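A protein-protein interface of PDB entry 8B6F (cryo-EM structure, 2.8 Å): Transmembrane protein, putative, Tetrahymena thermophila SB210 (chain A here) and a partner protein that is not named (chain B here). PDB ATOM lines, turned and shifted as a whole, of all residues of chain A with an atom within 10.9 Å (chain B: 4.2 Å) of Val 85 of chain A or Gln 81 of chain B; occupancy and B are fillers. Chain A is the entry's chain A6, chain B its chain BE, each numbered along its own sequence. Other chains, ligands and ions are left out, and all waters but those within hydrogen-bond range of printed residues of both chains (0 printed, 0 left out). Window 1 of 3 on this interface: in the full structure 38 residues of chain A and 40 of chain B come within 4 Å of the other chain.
The side-chain amino group (NZ) of Lys 108 of chain B lies within hydrogen-bond range of the side-chain amide oxygen (OE1) of Gln 81 of chain B, at 2.5 Å. OE1 of Glu 151 of chain B lies within salt-bridge range of NZ of Lys 108 of chain B (2.6 Å). N of Cys 99 of chain B is in hydrogen-bond range of O of Leu 106 of chain B (2.8 Å). SG of Cys 99 of chain B is in hydrogen-bond range of OE1 of Gln 81 of chain B, 3.6 Å away. The side-chain amide oxygen (OE1) of Gln 81 of chain B sits close to the side-chain carboxylate (OE2) of Glu 151 of chain B, at 3.0 Å. The backbone carbonyl oxygen (O) of Gln 81 of chain B sits at hydrogen-bond distance from the backbone NH (N) of Val 154 of chain B, 3.0 Å away.
Printed residues of chain B within 4 Å of Asn 82 of chain A: Leu 106. Val 85 of chain A touches just these residues of chain B: Gln 81 and Leu 106. Printed residues of chain B within 4 Å of Ser 86 of chain A: Lys 108. Of the printed residues of chain B, Thr 87 of chain A touches Lys 108 (3.3 Å). Of the printed residues of chain A, Gln 81 of chain B touches Val 85. No residue of chain A comes within 4 Å of Cys 99 of chain B. Of the printed residues of chain A, Leu 106 of chain B touches Asn 82 (3.8 Å) and Val 85 (3.3 Å). Phe 152 of chain B touches none of the printed residues of chain A. No residue of chain A comes within 4 Å of Val 154 of chain B. The nearest printed residue of chain B that does not touch Val 85 of chain A is Lys 108 of chain B (4.6 Å). The nearest residue of chain A that does not touch Gln 81 of chain B is Ser 86 of chain A (5.2 Å).
Printed residues of chain A that touch a printed residue of chain B: Asn 82, Val 85, Ser 86 and Thr 87. Hydrophobic or aromatic side chains of chain A that line the printed part of chain B: Val 85. Hydrophobic or aromatic side chains of chain B within 4 Å of the printed part of chain A: Leu 106. Among the printed residues, 5 pairs touch across the chains. Among the printed residues, no Asp or Glu carboxylate lies within 4 Å of a Lys or Arg side-chain nitrogen of the other chain.
Among the printed residues, pairs that only touch across the chains: Ser 86 of chain A with Lys 108 of chain B, Thr 87 of chain A with Lys 108 of chain B, Val 85 of chain A with Leu 106 of chain B, Val 85 of chain A with Gln 81 of chain B and Asn 82 of chain A with Leu 106 of chain B.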
ATOM      1  N   LEU A  79       6.744  19.642 -10.317  1.00  0.00           N
ATOM      2  CA  LEU A  79       6.562  19.959 -11.730  1.00  0.00           C
ATOM      3  C   LEU A  79       5.514  21.054 -11.893  1.00  0.00           C
ATOM      4  O   LEU A  79       4.962  21.543 -10.903  1.00  0.00           O
ATOM      5  CB  LEU A  79       6.173  18.712 -12.525  1.00  0.00           C
ATOM      6  CG  LEU A  79       7.227  18.159 -13.493  1.00  0.00           C
ATOM      7  CD1 LEU A  79       6.707  16.902 -14.175  1.00  0.00           C
ATOM      8  CD2 LEU A  79       7.639  19.195 -14.537  1.00  0.00           C
ATOM      9  N   ASP A  80       5.242  21.449 -13.137  1.00  0.00           N
ATOM     10  CA  ASP A  80       4.271  22.504 -13.404  1.00  0.00           C
ATOM     11  C   ASP A  80       2.935  22.190 -12.742  1.00  0.00           C
ATOM     12  O   ASP A  80       2.425  21.071 -12.839  1.00  0.00           O
ATOM     13  CB  ASP A  80       4.089  22.666 -14.914  1.00  0.00           C
ATOM     14  CG  ASP A  80       3.102  23.760 -15.271  1.00  0.00           C
ATOM     15  OD1 ASP A  80       2.654  24.487 -14.360  1.00  0.00           O
ATOM     16  OD2 ASP A  80       2.771  23.893 -16.467  1.00  0.00           O
ATOM     17  N   THR A  81       2.364  23.191 -12.077  1.00  0.00           N
ATOM     18  CA  THR A  81       1.150  23.013 -11.294  1.00  0.00           C
ATOM     19  C   THR A  81      -0.097  23.228 -12.141  1.00  0.00           C
ATOM     20  O   THR A  81      -0.086  23.969 -13.127  1.00  0.00           O
ATOM     21  CB  THR A  81       1.119  23.973 -10.106  1.00  0.00           C
ATOM     22  OG1 THR A  81       1.288  25.319 -10.568  1.00  0.00           O
ATOM     23  CG2 THR A  81       2.215  23.631  -9.117  1.00  0.00           C
ATOM     24  N   ASN A  82      -1.183  22.567 -11.737  1.00  0.00           N
ATOM     25  CA  ASN A  82      -2.467  22.750 -12.403  1.00  0.00           C
ATOM     26  C   ASN A  82      -3.109  24.087 -12.062  1.00  0.00           C
ATOM     27  O   ASN A  82      -4.012  24.527 -12.781  1.00  0.00           O
ATOM     28  CB  ASN A  82      -3.420  21.615 -12.025  1.00  0.00           C
ATOM     29  CG  ASN A  82      -2.939  20.264 -12.511  1.00  0.00           C
ATOM     30  OD1 ASN A  82      -1.818  20.130 -12.998  1.00  0.00           O
ATOM     31  ND2 ASN A  82      -3.786  19.251 -12.375  1.00  0.00           N
ATOM     32  N   SER A  83      -2.674  24.738 -10.982  1.00  0.00           N
ATOM     33  CA  SER A  83      -3.277  26.008 -10.594  1.00  0.00           C
ATOM     34  C   SER A  83      -3.071  27.067 -11.668  1.00  0.00           C
ATOM     35  O   SER A  83      -3.990  27.829 -11.983  1.00  0.00           O
ATOM     36  CB  SER A  83      -2.699  26.478  -9.259  1.00  0.00           C
ATOM     37  OG  SER A  83      -1.301  26.685  -9.352  1.00  0.00           O
ATOM     38  N   ALA A  84      -1.867  27.135 -12.240  1.00  0.00           N
ATOM     39  CA  ALA A  84      -1.582  28.112 -13.284  1.00  0.00           C
ATOM     40  C   ALA A  84      -2.228  27.761 -14.616  1.00  0.00           C
ATOM     41  O   ALA A  84      -2.257  28.612 -15.510  1.00  0.00           O
ATOM     42  CB  ALA A  84      -0.072  28.251 -13.473  1.00  0.00           C
ATOM     43  N   VAL A  85      -2.733  26.539 -14.775  1.00  0.00           N
ATOM     44  CA  VAL A  85      -3.384  26.154 -16.021  1.00  0.00           C
ATOM     45  C   VAL A  85      -4.703  26.901 -16.147  1.00  0.00           C
ATOM     46  O   VAL A  85      -5.513  26.930 -15.212  1.00  0.00           O
ATOM     47  CB  VAL A  85      -3.595  24.634 -16.068  1.00  0.00           C
ATOM     48  CG1 VAL A  85      -4.354  24.230 -17.326  1.00  0.00           C
ATOM     49  CG2 VAL A  85      -2.260  23.913 -15.997  1.00  0.00           C
ATOM     50  N   SER A  86      -4.927  27.511 -17.308  1.00  0.00           N
ATOM     51  CA  SER A  86      -6.186  28.201 -17.550  1.00  0.00           C
ATOM     52  C   SER A  86      -7.339  27.209 -17.490  1.00  0.00           C
ATOM     53  O   SER A  86      -7.204  26.049 -17.889  1.00  0.00           O
ATOM     54  CB  SER A  86      -6.160  28.900 -18.908  1.00  0.00           C
ATOM     55  OG  SER A  86      -5.985  27.964 -19.956  1.00  0.00           O
ATOM     56  N   THR A  87      -8.479  27.671 -16.980  1.00  0.00           N
ATOM     57  CA  THR A  87      -9.640  26.817 -16.777  1.00  0.00           C
ATOM     58  C   THR A  87     -10.871  27.262 -17.552  1.00  0.00           C
ATOM     59  O   THR A  87     -11.918  26.618 -17.437  1.00  0.00           O
ATOM     60  CB  THR A  87      -9.987  26.747 -15.282  1.00  0.00           C
ATOM     61  OG1 THR A  87     -11.144  25.925 -15.091  1.00  0.00           O
ATOM     62  CG2 THR A  87     -10.260  28.135 -14.725  1.00  0.00           C
ATOM     63  N   SER A  88     -10.786  28.337 -18.331  1.00  0.00           N
ATOM     64  CA  SER A  88     -11.943  28.818 -19.070  1.00  0.00           C
ATOM     65  C   SER A  88     -11.470  29.691 -20.221  1.00  0.00           C
ATOM     66  O   SER A  88     -10.323  30.143 -20.251  1.00  0.00           O
ATOM     67  CB  SER A  88     -12.899  29.597 -18.162  1.00  0.00           C
ATOM     68  OG  SER A  88     -14.015  30.081 -18.889  1.00  0.00           O
ATOM     69  N   ASP A  89     -12.375  29.921 -21.170  1.00  0.00           N
ATOM     70  CA  ASP A  89     -12.110  30.814 -22.290  1.00  0.00           C
ATOM     71  C   ASP A  89     -12.346  32.277 -21.945  1.00  0.00           C
ATOM     72  O   ASP A  89     -12.103  33.142 -22.794  1.00  0.00           O
ATOM     73  CB  ASP A  89     -12.977  30.430 -23.492  1.00  0.00           C
ATOM     74  CG  ASP A  89     -12.556  29.115 -24.119  1.00  0.00           C
ATOM     75  OD1 ASP A  89     -11.643  28.461 -23.575  1.00  0.00           O
ATOM     76  OD2 ASP A  89     -13.135  28.741 -25.160  1.00  0.00           O
ATOM     77  N   PHE A  90     -12.816  32.572 -20.738  1.00  0.00           N
ATOM     78  CA  PHE A  90     -13.018  33.937 -20.274  1.00  0.00           C
ATOM     79  C   PHE A  90     -12.024  34.232 -19.161  1.00  0.00           C
ATOM     80  O   PHE A  90     -11.918  33.463 -18.200  1.00  0.00           O
ATOM     81  CB  PHE A  90     -14.451  34.140 -19.779  1.00  0.00           C
ATOM     82  CG  PHE A  90     -14.663  35.441 -19.065  1.00  0.00           C
ATOM     83  CD1 PHE A  90     -14.831  36.617 -19.775  1.00  0.00           C
ATOM     84  CD2 PHE A  90     -14.699  35.486 -17.683  1.00  0.00           C
ATOM     85  CE1 PHE A  90     -15.027  37.816 -19.118  1.00  0.00           C
ATOM     86  CE2 PHE A  90     -14.896  36.680 -17.021  1.00  0.00           C
ATOM     87  CZ  PHE A  90     -15.060  37.847 -17.739  1.00  0.00           C
ATOM     88  N   VAL A  91     -11.301  35.340 -19.293  1.00  0.00           N
ATOM     89  CA  VAL A  91     -10.271  35.734 -18.341  1.00  0.00           C
ATOM     90  C   VAL A  91     -10.605  37.122 -17.822  1.00  0.00           C
ATOM     91  O   VAL A  91     -10.924  38.025 -18.605  1.00  0.00           O
ATOM     92  CB  VAL A  91      -8.869  35.715 -18.978  1.00  0.00           C
ATOM     93  CG1 VAL A  91      -7.807  35.990 -17.925  1.00  0.00           C
ATOM     94  CG2 VAL A  91      -8.611  34.383 -19.665  1.00  0.00           C
ATOM     95  N   ARG A 107      -1.129  37.155 -23.854  1.00  0.00           N
ATOM     96  CA  ARG A 107      -0.938  35.894 -23.144  1.00  0.00           C
ATOM     97  C   ARG A 107       0.466  35.321 -23.306  1.00  0.00           C
ATOM     98  O   ARG A 107       1.188  35.156 -22.319  1.00  0.00           O
ATOM     99  CB  ARG A 107      -1.978  34.871 -23.617  1.00  0.00           C
ATOM    100  CG  ARG A 107      -3.404  35.240 -23.256  1.00  0.00           C
ATOM    101  CD  ARG A 107      -4.375  34.148 -23.659  1.00  0.00           C
ATOM    102  NE  ARG A 107      -4.421  33.964 -25.104  1.00  0.00           N
ATOM    103  CZ  ARG A 107      -5.225  33.113 -25.725  1.00  0.00           C
ATOM    104  NH1 ARG A 107      -6.069  32.344 -25.056  1.00  0.00           N
ATOM    105  NH2 ARG A 107      -5.182  33.029 -27.051  1.00  0.00           N
ATOM    106  N   LYS B  73       4.131  17.785 -22.594  1.00  0.00           N
ATOM    107  CA  LYS B  73       3.390  18.993 -22.241  1.00  0.00           C
ATOM    108  C   LYS B  73       4.315  20.043 -21.642  1.00  0.00           C
ATOM    109  O   LYS B  73       4.252  21.224 -21.999  1.00  0.00           O
ATOM    110  CB  LYS B  73       2.279  18.664 -21.241  1.00  0.00           C
ATOM    111  CG  LYS B  73       1.087  17.909 -21.793  1.00  0.00           C
ATOM    112  CD  LYS B  73      -0.043  17.930 -20.769  1.00  0.00           C
ATOM    113  CE  LYS B  73      -1.091  16.870 -21.051  1.00  0.00           C
ATOM    114  NZ  LYS B  73      -2.208  16.924 -20.064  1.00  0.00           N
ATOM    115  N   LYS B  80      -1.408  20.514 -24.964  1.00  0.00           N
ATOM    116  CA  LYS B  80      -2.312  19.392 -25.159  1.00  0.00           C
ATOM    117  C   LYS B  80      -2.822  18.933 -23.803  1.00  0.00           C
ATOM    118  O   LYS B  80      -2.196  19.180 -22.769  1.00  0.00           O
ATOM    119  CB  LYS B  80      -1.619  18.242 -25.896  1.00  0.00           C
ATOM    120  CG  LYS B  80      -0.392  17.707 -25.180  1.00  0.00           C
ATOM    121  CD  LYS B  80       0.393  16.763 -26.071  1.00  0.00           C
ATOM    122  CE  LYS B  80       1.528  16.107 -25.310  1.00  0.00           C
ATOM    123  NZ  LYS B  80       2.271  15.138 -26.157  1.00  0.00           N
ATOM    124  N   GLN B  81      -3.974  18.266 -23.812  1.00  0.00           N
ATOM    125  CA  GLN B  81      -4.574  17.782 -22.575  1.00  0.00           C
ATOM    126  C   GLN B  81      -5.307  16.474 -22.823  1.00  0.00           C
ATOM    127  O   GLN B  81      -6.069  16.353 -23.787  1.00  0.00           O
ATOM    128  CB  GLN B  81      -5.525  18.821 -21.977  1.00  0.00           C
ATOM    129  CG  GLN B  81      -4.806  19.876 -21.158  1.00  0.00           C
ATOM    130  CD  GLN B  81      -5.747  20.905 -20.583  1.00  0.00           C
ATOM    131  OE1 GLN B  81      -6.768  21.232 -21.184  1.00  0.00           O
ATOM    132  NE2 GLN B  81      -5.412  21.420 -19.407  1.00  0.00           N
ATOM    133  N   PHE B  82      -5.070  15.506 -21.942  1.00  0.00           N
ATOM    134  CA  PHE B  82      -5.767  14.226 -21.958  1.00  0.00           C
ATOM    135  C   PHE B  82      -7.112  14.412 -21.265  1.00  0.00           C
ATOM    136  O   PHE B  82      -7.165  14.685 -20.063  1.00  0.00           O
ATOM    137  CB  PHE B  82      -4.914  13.166 -21.265  1.00  0.00           C
ATOM    138  CG  PHE B  82      -5.464  11.777 -21.365  1.00  0.00           C
ATOM    139  CD1 PHE B  82      -5.299  11.035 -22.523  1.00  0.00           C
ATOM    140  CD2 PHE B  82      -6.120  11.199 -20.292  1.00  0.00           C
ATOM    141  CE1 PHE B  82      -5.794   9.752 -22.616  1.00  0.00           C
ATOM    142  CE2 PHE B  82      -6.617   9.916 -20.378  1.00  0.00           C
ATOM    143  CZ  PHE B  82      -6.454   9.190 -21.541  1.00  0.00           C
ATOM    144  N   VAL B  83      -8.199  14.264 -22.018  1.00  0.00           N
ATOM    145  CA  VAL B  83      -9.533  14.644 -21.566  1.00  0.00           C
ATOM    146  C   VAL B  83     -10.290  13.404 -21.119  1.00  0.00           C
ATOM    147  O   VAL B  83     -10.265  12.369 -21.796  1.00  0.00           O
ATOM    148  CB  VAL B  83     -10.304  15.381 -22.673  1.00  0.00           C
ATOM    149  CG1 VAL B  83     -11.724  15.700 -22.227  1.00  0.00           C
ATOM    150  CG2 VAL B  83      -9.575  16.649 -23.069  1.00  0.00           C
ATOM    151  N   CYS B  99      -9.551  17.018 -17.195  1.00  0.00           N
ATOM    152  CA  CYS B  99      -8.284  16.663 -17.813  1.00  0.00           C
ATOM    153  C   CYS B  99      -7.333  16.109 -16.764  1.00  0.00           C
ATOM    154  O   CYS B  99      -7.284  16.603 -15.634  1.00  0.00           O
ATOM    155  CB  CYS B  99      -7.655  17.879 -18.496  1.00  0.00           C
ATOM    156  SG  CYS B  99      -8.783  18.762 -19.593  1.00  0.00           S
ATOM    157  N   LEU B 106      -8.074  18.263 -13.419  1.00  0.00           N
ATOM    158  CA  LEU B 106      -8.385  19.678 -13.527  1.00  0.00           C
ATOM    159  C   LEU B 106      -9.653  19.855 -14.351  1.00  0.00           C
ATOM    160  O   LEU B 106      -9.943  19.058 -15.247  1.00  0.00           O
ATOM    161  CB  LEU B 106      -7.227  20.446 -14.174  1.00  0.00           C
ATOM    162  CG  LEU B 106      -7.431  21.945 -14.394  1.00  0.00           C
ATOM    163  CD1 LEU B 106      -7.628  22.669 -13.070  1.00  0.00           C
ATOM    164  CD2 LEU B 106      -6.253  22.525 -15.158  1.00  0.00           C
ATOM    165  N   LYS B 108     -11.855  22.306 -16.892  1.00  0.00           N
ATOM    166  CA  LYS B 108     -11.711  23.367 -17.873  1.00  0.00           C
ATOM    167  C   LYS B 108     -13.035  23.559 -18.600  1.00  0.00           C
ATOM    168  O   LYS B 108     -13.836  22.629 -18.714  1.00  0.00           O
ATOM    169  CB  LYS B 108     -10.590  23.047 -18.876  1.00  0.00           C
ATOM    170  CG  LYS B 108     -10.407  24.099 -19.962  1.00  0.00           C
ATOM    171  CD  LYS B 108      -9.257  23.757 -20.895  1.00  0.00           C
ATOM    172  CE  LYS B 108      -7.918  23.861 -20.193  1.00  0.00           C
ATOM    173  NZ  LYS B 108      -6.785  23.738 -21.150  1.00  0.00           N
ATOM    174  N   GLU B 151      -4.772  25.065 -28.232  1.00  0.00           N
ATOM    175  CA  GLU B 151      -4.531  23.867 -27.445  1.00  0.00           C
ATOM    176  C   GLU B 151      -5.192  22.673 -28.120  1.00  0.00           C
ATOM    177  O   GLU B 151      -6.114  22.821 -28.925  1.00  0.00           O
ATOM    178  CB  GLU B 151      -5.056  24.041 -26.016  1.00  0.00           C
ATOM    179  CG  GLU B 151      -4.610  22.971 -25.046  1.00  0.00           C
ATOM    180  CD  GLU B 151      -5.004  23.297 -23.623  1.00  0.00           C
ATOM    181  OE1 GLU B 151      -5.762  24.269 -23.429  1.00  0.00           O
ATOM    182  OE2 GLU B 151      -4.554  22.589 -22.700  1.00  0.00           O
ATOM    183  N   PHE B 152      -4.714  21.482 -27.773  1.00  0.00           N
ATOM    184  CA  PHE B 152      -5.239  20.228 -28.293  1.00  0.00           C
ATOM    185  C   PHE B 152      -5.901  19.429 -27.181  1.00  0.00           C
ATOM    186  O   PHE B 152      -5.452  19.454 -26.031  1.00  0.00           O
ATOM    187  CB  PHE B 152      -4.132  19.389 -28.934  1.00  0.00           C
ATOM    188  CG  PHE B 152      -3.525  20.018 -30.149  1.00  0.00           C
ATOM    189  CD1 PHE B 152      -2.461  20.893 -30.032  1.00  0.00           C
ATOM    190  CD2 PHE B 152      -4.019  19.737 -31.411  1.00  0.00           C
ATOM    191  CE1 PHE B 152      -1.901  21.475 -31.148  1.00  0.00           C
ATOM    192  CE2 PHE B 152      -3.465  20.317 -32.533  1.00  0.00           C
ATOM    193  CZ  PHE B 152      -2.403  21.187 -32.401  1.00  0.00           C
ATOM    194  N   TYR B 153      -6.973  18.723 -27.532  1.00  0.00           N
ATOM    195  CA  TYR B 153      -7.662  17.811 -26.627  1.00  0.00           C
ATOM    196  C   TYR B 153      -7.588  16.409 -27.210  1.00  0.00           C
ATOM    197  O   TYR B 153      -8.001  16.186 -28.352  1.00  0.00           O
ATOM    198  CB  TYR B 153      -9.116  18.228 -26.417  1.00  0.00           C
ATOM    199  CG  TYR B 153      -9.276  19.622 -25.867  1.00  0.00           C
ATOM    200  CD1 TYR B 153      -8.661  19.992 -24.680  1.00  0.00           C
ATOM    201  CD2 TYR B 153     -10.053  20.561 -26.524  1.00  0.00           C
ATOM    202  CE1 TYR B 153      -8.805  21.261 -24.169  1.00  0.00           C
ATOM    203  CE2 TYR B 153     -10.204  21.834 -26.022  1.00  0.00           C
ATOM    204  CZ  TYR B 153      -9.580  22.178 -24.844  1.00  0.00           C
ATOM    205  OH  TYR B 153      -9.732  23.447 -24.340  1.00  0.00           O
ATOM    206  N   VAL B 154      -7.074  15.468 -26.423  1.00  0.00           N
ATOM    207  CA  VAL B 154      -6.899  14.085 -26.846  1.00  0.00           C
ATOM    208  C   VAL B 154      -7.703  13.200 -25.906  1.00  0.00           C
ATOM    209  O   VAL B 154      -7.569  13.303 -24.682  1.00  0.00           O
ATOM    210  CB  VAL B 154      -5.415  13.675 -26.845  1.00  0.00           C
ATOM    211  CG1 VAL B 154      -5.252  12.253 -27.360  1.00  0.00           C
ATOM    212  CG2 VAL B 154      -4.589  14.649 -27.671  1.00  0.00           C
